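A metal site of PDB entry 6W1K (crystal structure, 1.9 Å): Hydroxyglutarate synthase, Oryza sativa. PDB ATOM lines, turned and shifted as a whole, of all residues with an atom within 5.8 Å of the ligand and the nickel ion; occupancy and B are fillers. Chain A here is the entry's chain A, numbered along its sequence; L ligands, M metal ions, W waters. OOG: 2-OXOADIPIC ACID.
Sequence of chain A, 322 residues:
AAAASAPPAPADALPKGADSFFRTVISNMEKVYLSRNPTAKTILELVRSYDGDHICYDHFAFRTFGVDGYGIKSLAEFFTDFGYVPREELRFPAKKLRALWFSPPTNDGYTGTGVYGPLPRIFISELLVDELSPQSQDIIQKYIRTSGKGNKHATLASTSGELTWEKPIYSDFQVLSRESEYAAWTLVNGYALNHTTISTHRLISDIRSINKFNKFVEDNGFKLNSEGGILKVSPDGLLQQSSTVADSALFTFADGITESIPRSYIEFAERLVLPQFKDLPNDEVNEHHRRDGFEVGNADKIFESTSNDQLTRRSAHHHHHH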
ATOM      1  N   HIS A  59       4.422  12.739  22.391  1.00  0.00           N
ATOM      2  CA  HIS A  59       4.056  12.272  21.066  1.00  0.00           C
ATOM      3  C   HIS A  59       2.542  12.366  20.833  1.00  0.00           C
ATOM      4  O   HIS A  59       1.743  12.503  21.768  1.00  0.00           O
ATOM      5  CB  HIS A  59       4.536  10.828  20.828  1.00  0.00           C
ATOM      6  CG  HIS A  59       3.933   9.808  21.743  1.00  0.00           C
ATOM      7  ND1 HIS A  59       4.432   9.538  22.991  1.00  0.00           N
ATOM      8  CD2 HIS A  59       2.886   8.944  21.572  1.00  0.00           C
ATOM      9  CE1 HIS A  59       3.723   8.573  23.560  1.00  0.00           C
ATOM     10  NE2 HIS A  59       2.787   8.186  22.716  1.00  0.00           N
ATOM     11  N   ALA A  61      -0.466  10.190  18.521  1.00  0.00           N
ATOM     12  CA  ALA A  61      -0.643   8.852  17.950  1.00  0.00           C
ATOM     13  C   ALA A  61      -1.909   8.809  17.077  1.00  0.00           C
ATOM     14  O   ALA A  61      -2.875   9.531  17.340  1.00  0.00           O
ATOM     15  CB  ALA A  61      -0.698   7.772  19.027  1.00  0.00           C
ATOM     16  N   PHE A  62      -1.845   8.044  15.986  1.00  0.00           N
ATOM     17  CA  PHE A  62      -2.927   7.919  15.015  1.00  0.00           C
ATOM     18  C   PHE A  62      -3.093   6.442  14.647  1.00  0.00           C
ATOM     19  O   PHE A  62      -2.131   5.681  14.695  1.00  0.00           O
ATOM     20  CB  PHE A  62      -2.671   8.726  13.717  1.00  0.00           C
ATOM     21  CG  PHE A  62      -2.449  10.205  13.932  1.00  0.00           C
ATOM     22  CD1 PHE A  62      -1.174  10.693  14.217  1.00  0.00           C
ATOM     23  CD2 PHE A  62      -3.495  11.087  13.862  1.00  0.00           C
ATOM     24  CE1 PHE A  62      -1.001  12.045  14.424  1.00  0.00           C
ATOM     25  CE2 PHE A  62      -3.335  12.450  14.062  1.00  0.00           C
ATOM     26  CZ  PHE A  62      -2.073  12.926  14.322  1.00  0.00           C
ATOM     27  N   ARG A  63      -4.326   6.077  14.248  1.00  0.00           N
ATOM     28  CA  ARG A  63      -4.672   4.725  13.831  1.00  0.00           C
ATOM     29  C   ARG A  63      -5.231   4.719  12.412  1.00  0.00           C
ATOM     30  O   ARG A  63      -5.903   5.673  11.987  1.00  0.00           O
ATOM     31  CB  ARG A  63      -5.704   4.121  14.775  1.00  0.00           C
ATOM     32  CG  ARG A  63      -5.218   4.003  16.208  1.00  0.00           C
ATOM     33  CD  ARG A  63      -6.212   3.239  17.065  1.00  0.00           C
ATOM     34  NE  ARG A  63      -5.720   3.086  18.431  1.00  0.00           N
ATOM     35  CZ  ARG A  63      -6.451   2.572  19.412  1.00  0.00           C
ATOM     36  NH1 ARG A  63      -7.698   2.172  19.166  1.00  0.00           N
ATOM     37  NH2 ARG A  63      -5.962   2.481  20.624  1.00  0.00           N
ATOM     38  N   PHE A 123       3.487   8.747  16.340  1.00  0.00           N
ATOM     39  CA  PHE A 123       3.355   7.293  16.364  1.00  0.00           C
ATOM     40  C   PHE A 123       2.139   6.965  15.496  1.00  0.00           C
ATOM     41  O   PHE A 123       1.043   7.453  15.782  1.00  0.00           O
ATOM     42  CB  PHE A 123       3.179   6.788  17.813  1.00  0.00           C
ATOM     43  CG  PHE A 123       3.174   5.293  17.960  1.00  0.00           C
ATOM     44  CD1 PHE A 123       2.049   4.536  17.630  1.00  0.00           C
ATOM     45  CD2 PHE A 123       4.294   4.640  18.465  1.00  0.00           C
ATOM     46  CE1 PHE A 123       2.052   3.137  17.784  1.00  0.00           C
ATOM     47  CE2 PHE A 123       4.309   3.256  18.621  1.00  0.00           C
ATOM     48  CZ  PHE A 123       3.195   2.506  18.283  1.00  0.00           C
ATOM     49  N   SER A 125       0.025   3.829  13.590  1.00  0.00           N
ATOM     50  CA  SER A 125      -0.165   2.390  13.457  1.00  0.00           C
ATOM     51  C   SER A 125      -1.156   2.137  12.326  1.00  0.00           C
ATOM     52  O   SER A 125      -1.875   3.041  11.880  1.00  0.00           O
ATOM     53  CB  SER A 125      -0.617   1.787  14.782  1.00  0.00           C
ATOM     54  OG  SER A 125      -1.824   2.346  15.197  1.00  0.00           O
ATOM     55  N   TYR A 182      -9.585  -2.532  17.521  1.00  0.00           N
ATOM     56  CA  TYR A 182      -8.876  -1.506  16.789  1.00  0.00           C
ATOM     57  C   TYR A 182      -9.634  -1.130  15.528  1.00  0.00           C
ATOM     58  O   TYR A 182      -9.808   0.055  15.214  1.00  0.00           O
ATOM     59  CB  TYR A 182      -7.477  -2.013  16.473  1.00  0.00           C
ATOM     60  CG  TYR A 182      -6.555  -1.030  15.756  1.00  0.00           C
ATOM     61  CD1 TYR A 182      -6.754  -0.717  14.422  1.00  0.00           C
ATOM     62  CD2 TYR A 182      -5.477  -0.462  16.417  1.00  0.00           C
ATOM     63  CE1 TYR A 182      -5.944   0.154  13.757  1.00  0.00           C
ATOM     64  CE2 TYR A 182      -4.637   0.425  15.750  1.00  0.00           C
ATOM     65  CZ  TYR A 182      -4.864   0.708  14.422  1.00  0.00           C
ATOM     66  OH  TYR A 182      -4.049   1.553  13.731  1.00  0.00           O
ATOM     67  N   ASN A 194      -5.554   9.982  18.196  1.00  0.00           N
ATOM     68  CA  ASN A 194      -5.961   8.920  19.131  1.00  0.00           C
ATOM     69  C   ASN A 194      -5.531   9.246  20.561  1.00  0.00           C
ATOM     70  O   ASN A 194      -6.250   8.930  21.522  1.00  0.00           O
ATOM     71  CB  ASN A 194      -5.366   7.595  18.666  1.00  0.00           C
ATOM     72  CG  ASN A 194      -5.520   6.513  19.683  1.00  0.00           C
ATOM     73  OD1 ASN A 194      -4.624   6.282  20.481  1.00  0.00           O
ATOM     74  ND2 ASN A 194      -6.667   5.858  19.685  1.00  0.00           N
ATOM     75  N   HIS A 195      -4.374   9.897  20.715  1.00  0.00           N
ATOM     76  CA  HIS A 195      -4.045  10.517  21.987  1.00  0.00           C
ATOM     77  C   HIS A 195      -2.865  11.465  21.814  1.00  0.00           C
ATOM     78  O   HIS A 195      -2.089  11.376  20.839  1.00  0.00           O
ATOM     79  CB  HIS A 195      -3.742   9.473  23.068  1.00  0.00           C
ATOM     80  CG  HIS A 195      -2.517   8.656  22.838  1.00  0.00           C
ATOM     81  ND1 HIS A 195      -2.522   7.474  22.099  1.00  0.00           N
ATOM     82  CD2 HIS A 195      -1.242   8.801  23.282  1.00  0.00           C
ATOM     83  CE1 HIS A 195      -1.313   6.961  22.091  1.00  0.00           C
ATOM     84  NE2 HIS A 195      -0.509   7.757  22.778  1.00  0.00           N
ATOM     85  N   THR A 197       0.279  12.930  24.580  1.00  0.00           N
ATOM     86  CA  THR A 197       1.060  12.389  25.694  1.00  0.00           C
ATOM     87  C   THR A 197       1.750  13.530  26.404  1.00  0.00           C
ATOM     88  O   THR A 197       2.452  14.305  25.757  1.00  0.00           O
ATOM     89  CB  THR A 197       2.110  11.416  25.171  1.00  0.00           C
ATOM     90  OG1 THR A 197       1.482  10.462  24.331  1.00  0.00           O
ATOM     91  CG2 THR A 197       2.821  10.698  26.289  1.00  0.00           C
ATOM     92  N   GLN A 241       5.230   4.447  31.109  1.00  0.00           N
ATOM     93  CA  GLN A 241       4.069   5.048  30.466  1.00  0.00           C
ATOM     94  C   GLN A 241       2.802   4.648  31.193  1.00  0.00           C
ATOM     95  O   GLN A 241       2.701   3.530  31.692  1.00  0.00           O
ATOM     96  CB  GLN A 241       3.992   4.637  29.017  1.00  0.00           C
ATOM     97  CG  GLN A 241       5.157   5.111  28.149  1.00  0.00           C
ATOM     98  CD  GLN A 241       5.132   4.467  26.783  1.00  0.00           C
ATOM     99  OE1 GLN A 241       5.749   3.428  26.548  1.00  0.00           O
ATOM    100  NE2 GLN A 241       4.419   5.095  25.866  1.00  0.00           N
ATOM    101  N   TYR A 265      -8.036   9.103  24.306  1.00  0.00           N
ATOM    102  CA  TYR A 265      -7.551   9.072  25.670  1.00  0.00           C
ATOM    103  C   TYR A 265      -6.312   9.954  25.728  1.00  0.00           C
ATOM    104  O   TYR A 265      -5.949  10.596  24.731  1.00  0.00           O
ATOM    105  CB  TYR A 265      -7.253   7.652  26.140  1.00  0.00           C
ATOM    106  CG  TYR A 265      -6.142   6.905  25.394  1.00  0.00           C
ATOM    107  CD1 TYR A 265      -6.437   6.176  24.253  1.00  0.00           C
ATOM    108  CD2 TYR A 265      -4.828   6.903  25.848  1.00  0.00           C
ATOM    109  CE1 TYR A 265      -5.470   5.471  23.573  1.00  0.00           C
ATOM    110  CE2 TYR A 265      -3.845   6.198  25.163  1.00  0.00           C
ATOM    111  CZ  TYR A 265      -4.187   5.494  24.021  1.00  0.00           C
ATOM    112  OH  TYR A 265      -3.252   4.767  23.311  1.00  0.00           O
ATOM    113  N   GLU A 267      -2.179  10.052  27.353  1.00  0.00           N
ATOM    114  CA  GLU A 267      -1.085   9.272  27.913  1.00  0.00           C
ATOM    115  C   GLU A 267      -0.116  10.201  28.642  1.00  0.00           C
ATOM    116  O   GLU A 267      -0.101  11.425  28.439  1.00  0.00           O
ATOM    117  CB  GLU A 267      -0.407   8.457  26.802  1.00  0.00           C
ATOM    118  CG  GLU A 267       0.753   7.613  27.247  1.00  0.00           C
ATOM    119  CD  GLU A 267       1.640   7.180  26.073  1.00  0.00           C
ATOM    120  OE1 GLU A 267       1.086   6.784  25.043  1.00  0.00           O
ATOM    121  OE2 GLU A 267       2.889   7.249  26.183  1.00  0.00           O
ATOM    122  N   PHE A 294      10.146   3.988  21.491  1.00  0.00           N
ATOM    123  CA  PHE A 294       8.972   3.319  22.042  1.00  0.00           C
ATOM    124  C   PHE A 294       9.339   1.868  22.338  1.00  0.00           C
ATOM    125  O   PHE A 294      10.453   1.427  22.072  1.00  0.00           O
ATOM    126  CB  PHE A 294       7.792   3.438  21.086  1.00  0.00           C
ATOM    127  CG  PHE A 294       7.352   4.862  20.853  1.00  0.00           C
ATOM    128  CD1 PHE A 294       6.345   5.418  21.631  1.00  0.00           C
ATOM    129  CD2 PHE A 294       7.964   5.638  19.876  1.00  0.00           C
ATOM    130  CE1 PHE A 294       5.965   6.727  21.420  1.00  0.00           C
ATOM    131  CE2 PHE A 294       7.588   6.945  19.656  1.00  0.00           C
ATOM    132  CZ  PHE A 294       6.575   7.497  20.411  1.00  0.00           C
ATOM    133  N   GLU A 295       8.397   1.117  22.886  1.00  0.00           N
ATOM    134  CA  GLU A 295       8.686  -0.253  23.322  1.00  0.00           C
ATOM    135  C   GLU A 295       7.477  -1.117  23.054  1.00  0.00           C
ATOM    136  O   GLU A 295       6.368  -0.807  23.498  1.00  0.00           O
ATOM    137  CB  GLU A 295       9.082  -0.280  24.802  1.00  0.00           C
ATOM    138  CG  GLU A 295       9.977  -1.480  25.164  1.00  0.00           C
ATOM    139  CD  GLU A 295       9.142  -2.707  25.468  1.00  0.00           C
ATOM    140  OE1 GLU A 295       8.077  -2.533  26.085  1.00  0.00           O
ATOM    141  OE2 GLU A 295       9.541  -3.850  25.101  1.00  0.00           O
ATOM    142  N   ASN A 298       5.257  -2.180  26.129  1.00  0.00           N
ATOM    143  CA  ASN A 298       4.402  -1.100  26.601  1.00  0.00           C
ATOM    144  C   ASN A 298       3.253  -0.824  25.629  1.00  0.00           C
ATOM    145  O   ASN A 298       2.079  -0.813  26.003  1.00  0.00           O
ATOM    146  CB  ASN A 298       5.221   0.190  26.790  1.00  0.00           C
ATOM    147  CG  ASN A 298       6.226   0.083  27.926  1.00  0.00           C
ATOM    148  OD1 ASN A 298       6.401  -0.980  28.480  1.00  0.00           O
ATOM    149  ND2 ASN A 298       6.827   1.201  28.289  1.00  0.00           N
ATOM    150  N   ALA A 299       3.605  -0.536  24.376  1.00  0.00           N
ATOM    151  CA  ALA A 299       2.612  -0.128  23.409  1.00  0.00           C
ATOM    152  C   ALA A 299       1.478  -1.141  23.317  1.00  0.00           C
ATOM    153  O   ALA A 299       0.315  -0.751  23.203  1.00  0.00           O
ATOM    154  CB  ALA A 299       3.271   0.032  22.049  1.00  0.00           C
ATOM    155  N   ASP A 300       1.818  -2.431  23.345  1.00  0.00           N
ATOM    156  CA  ASP A 300       0.810  -3.474  23.211  1.00  0.00           C
ATOM    157  C   ASP A 300      -0.321  -3.275  24.222  1.00  0.00           C
ATOM    158  O   ASP A 300      -1.485  -3.472  23.885  1.00  0.00           O
ATOM    159  CB  ASP A 300       1.429  -4.866  23.378  1.00  0.00           C
ATOM    160  CG  ASP A 300       0.493  -6.005  22.962  1.00  0.00           C
ATOM    161  OD1 ASP A 300      -0.309  -5.842  22.017  1.00  0.00           O
ATOM    162  OD2 ASP A 300       0.564  -7.083  23.577  1.00  0.00           O
ATOM    163  N   ILE A 302      -1.006  -0.354  25.967  1.00  0.00           N
ATOM    164  CA  ILE A 302      -1.584   0.979  25.892  1.00  0.00           C
ATOM    165  C   ILE A 302      -2.658   1.028  24.816  1.00  0.00           C
ATOM    166  O   ILE A 302      -3.633   1.775  24.951  1.00  0.00           O
ATOM    167  CB  ILE A 302      -0.482   2.023  25.649  1.00  0.00           C
ATOM    168  CG1 ILE A 302       0.449   2.067  26.870  1.00  0.00           C
ATOM    169  CG2 ILE A 302      -1.054   3.425  25.411  1.00  0.00           C
ATOM    170  CD1 ILE A 302       1.725   2.880  26.650  1.00  0.00           C
ATOM    171  N   PHE A 303      -2.528   0.207  23.750  1.00  0.00           N
ATOM    172  CA  PHE A 303      -3.574   0.125  22.731  1.00  0.00           C
ATOM    173  C   PHE A 303      -4.936  -0.175  23.370  1.00  0.00           C
ATOM    174  O   PHE A 303      -5.983   0.169  22.818  1.00  0.00           O
ATOM    175  CB  PHE A 303      -3.291  -0.991  21.702  1.00  0.00           C
ATOM    176  CG  PHE A 303      -2.370  -0.582  20.575  1.00  0.00           C
ATOM    177  CD1 PHE A 303      -2.737   0.434  19.692  1.00  0.00           C
ATOM    178  CD2 PHE A 303      -1.151  -1.209  20.395  1.00  0.00           C
ATOM    179  CE1 PHE A 303      -1.887   0.822  18.661  1.00  0.00           C
ATOM    180  CE2 PHE A 303      -0.294  -0.826  19.368  1.00  0.00           C
ATOM    181  CZ  PHE A 303      -0.657   0.185  18.498  1.00  0.00           C
ATOM    182  N   GLU A 304      -4.926  -0.839  24.517  1.00  0.00           N
ATOM    183  CA  GLU A 304      -6.154  -1.294  25.139  1.00  0.00           C
ATOM    184  C   GLU A 304      -6.855  -0.215  25.955  1.00  0.00           C
ATOM    185  O   GLU A 304      -7.930  -0.477  26.526  1.00  0.00           O
ATOM    186  CB  GLU A 304      -5.847  -2.540  25.974  1.00  0.00           C
ATOM    187  CG  GLU A 304      -5.376  -3.709  25.095  1.00  0.00           C
ATOM    188  CD  GLU A 304      -5.224  -5.025  25.838  1.00  0.00           C
ATOM    189  OE1 GLU A 304      -6.051  -5.285  26.746  1.00  0.00           O
ATOM    190  OE2 GLU A 304      -4.280  -5.784  25.507  1.00  0.00           O
ATOM    191  N   THR A 306      -8.571   1.936  24.728  1.00  0.00           N
ATOM    192  CA  THR A 306      -9.844   2.115  24.062  1.00  0.00           C
ATOM    193  C   THR A 306     -10.687   0.846  24.055  1.00  0.00           C
ATOM    194  O   THR A 306     -11.796   0.867  23.494  1.00  0.00           O
ATOM    195  CB  THR A 306      -9.645   2.577  22.608  1.00  0.00           C
ATOM    196  OG1 THR A 306      -8.670   1.734  21.956  1.00  0.00           O
ATOM    197  CG2 THR A 306      -9.205   4.037  22.531  1.00  0.00           C
HETATM  198  C2  OOG L   1      -1.095   3.774  20.122  1.00  0.00           C
HETATM  199  C3  OOG L   1      -0.657   3.000  21.361  1.00  0.00           C
HETATM  200  C4  OOG L   1       0.874   2.905  21.404  1.00  0.00           C
HETATM  201  C6  OOG L   1       2.729   4.136  22.853  1.00  0.00           C
HETATM  202  O4  OOG L   1       3.477   3.132  22.827  1.00  0.00           O
HETATM  203  O3  OOG L   1       2.985   5.090  23.611  1.00  0.00           O
HETATM  204  C5  OOG L   1       1.502   4.197  21.943  1.00  0.00           C
HETATM  205  C1  OOG L   1      -2.616   3.705  19.905  1.00  0.00           C
HETATM  206  O1  OOG L   1      -3.088   3.966  18.854  1.00  0.00           O
HETATM  207  O2  OOG L   1      -3.477   3.324  20.941  1.00  0.00           O
HETATM  208  O5  OOG L   1       1.045   5.242  21.663  1.00  0.00           O
HETATM  209 NI    NI M   1       1.361   6.730  23.155  1.00  0.00          NI
HETATM  210  O   HOH W   1      -1.321   4.151  16.957  1.00  0.00           O
HETATM  211  O   HOH W   2       5.905   2.526  23.927  1.00  0.00           O
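Residues that only touch the ligand: Ala 299, Phe 303, Phe 123, Phe 294 and Ile 302.
Hydrophobic or aromatic side chains within 4 Å of the ligand: His 59, Phe 123, His 195, Tyr 265, Phe 294, Ala 299, Ile 302 and Phe 303.
Within 4 Å of the ligand: His 59, Arg 63, Phe 123, Asn 194, His 195, Gln 241, Tyr 265, Glu 267, Phe 294, Ala 299, Ile 302 and Phe 303.
Along chain A the residues within 4 Å of the ligand span positions 59 to 303.
The side-chain carboxylate (OE2) of Glu 267 lies within hydrogen-bond range of the side-chain amide nitrogen (NE2) of Gln 241 (2.7 Å).
The backbone carbonyl oxygen (O) of His 195 is in hydrogen-bond range of the backbone NH (N) of Ala 61 (3.1 Å).
ND1 of His 195 sits at hydrogen-bond distance from OH of Tyr 265.
The side-chain amide nitrogen of Asn 194 sits close to the guanidinium group of Arg 63 (3.2 Å).
The side-chain hydroxyl of Tyr 265 sits close to the backbone carbonyl oxygen of Ile 302 (3.4 Å).
The side-chain hydroxyl of Thr 306 sits at hydrogen-bond distance from the backbone carbonyl oxygen of Phe 303.
N of Asn 194 sits at hydrogen-bond distance from O of Ala 61 (2.8 Å).
The backbone NH of Thr 197 sits at hydrogen-bond distance from the backbone carbonyl oxygen of His 59 (3.2 Å).
The nickel ion is bound by OE1 of Glu 267 (1.9 Å), NE2 of His 59 (2.1 Å), O5 of the ligand (2.1 Å), NE2 of His 195 (2.2 Å) and O3 of the ligand (2.4 Å).
The nickel ion has five donor atoms within binding distance.
Water W1 lies within hydrogen-bond range of the side-chain hydroxyl (OG) of Ser 125, an oxygen (O1) of the ligand and the backbone carbonyl oxygen (O) of Phe 62.
Water W2 lies within hydrogen-bond range of an oxygen (O4) of the ligand, the side-chain amide oxygen of Gln 241 and the backbone NH of Glu 295.
The guanidinium group of Arg 63 is in salt-bridge range of an oxygen (O2) of the ligand, 2.6 Å away.
NE2 of Gln 241 sits close to O3 of the ligand (2.7 Å).
The side-chain amide oxygen of Asn 194 sits close to an oxygen (O2) of the ligand.
The side-chain hydroxyl of Tyr 265 is in hydrogen-bond range of an oxygen (O2) of the ligand.
OG1 of Thr 197 touches the nickel ion (3.9 Å).
Within 4 Å of the nickel ion: His 59, His 195, Thr 197 and Glu 267.
The nearest printed residue that does not touch the nickel ion is Gln 241 (4.4 Å).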
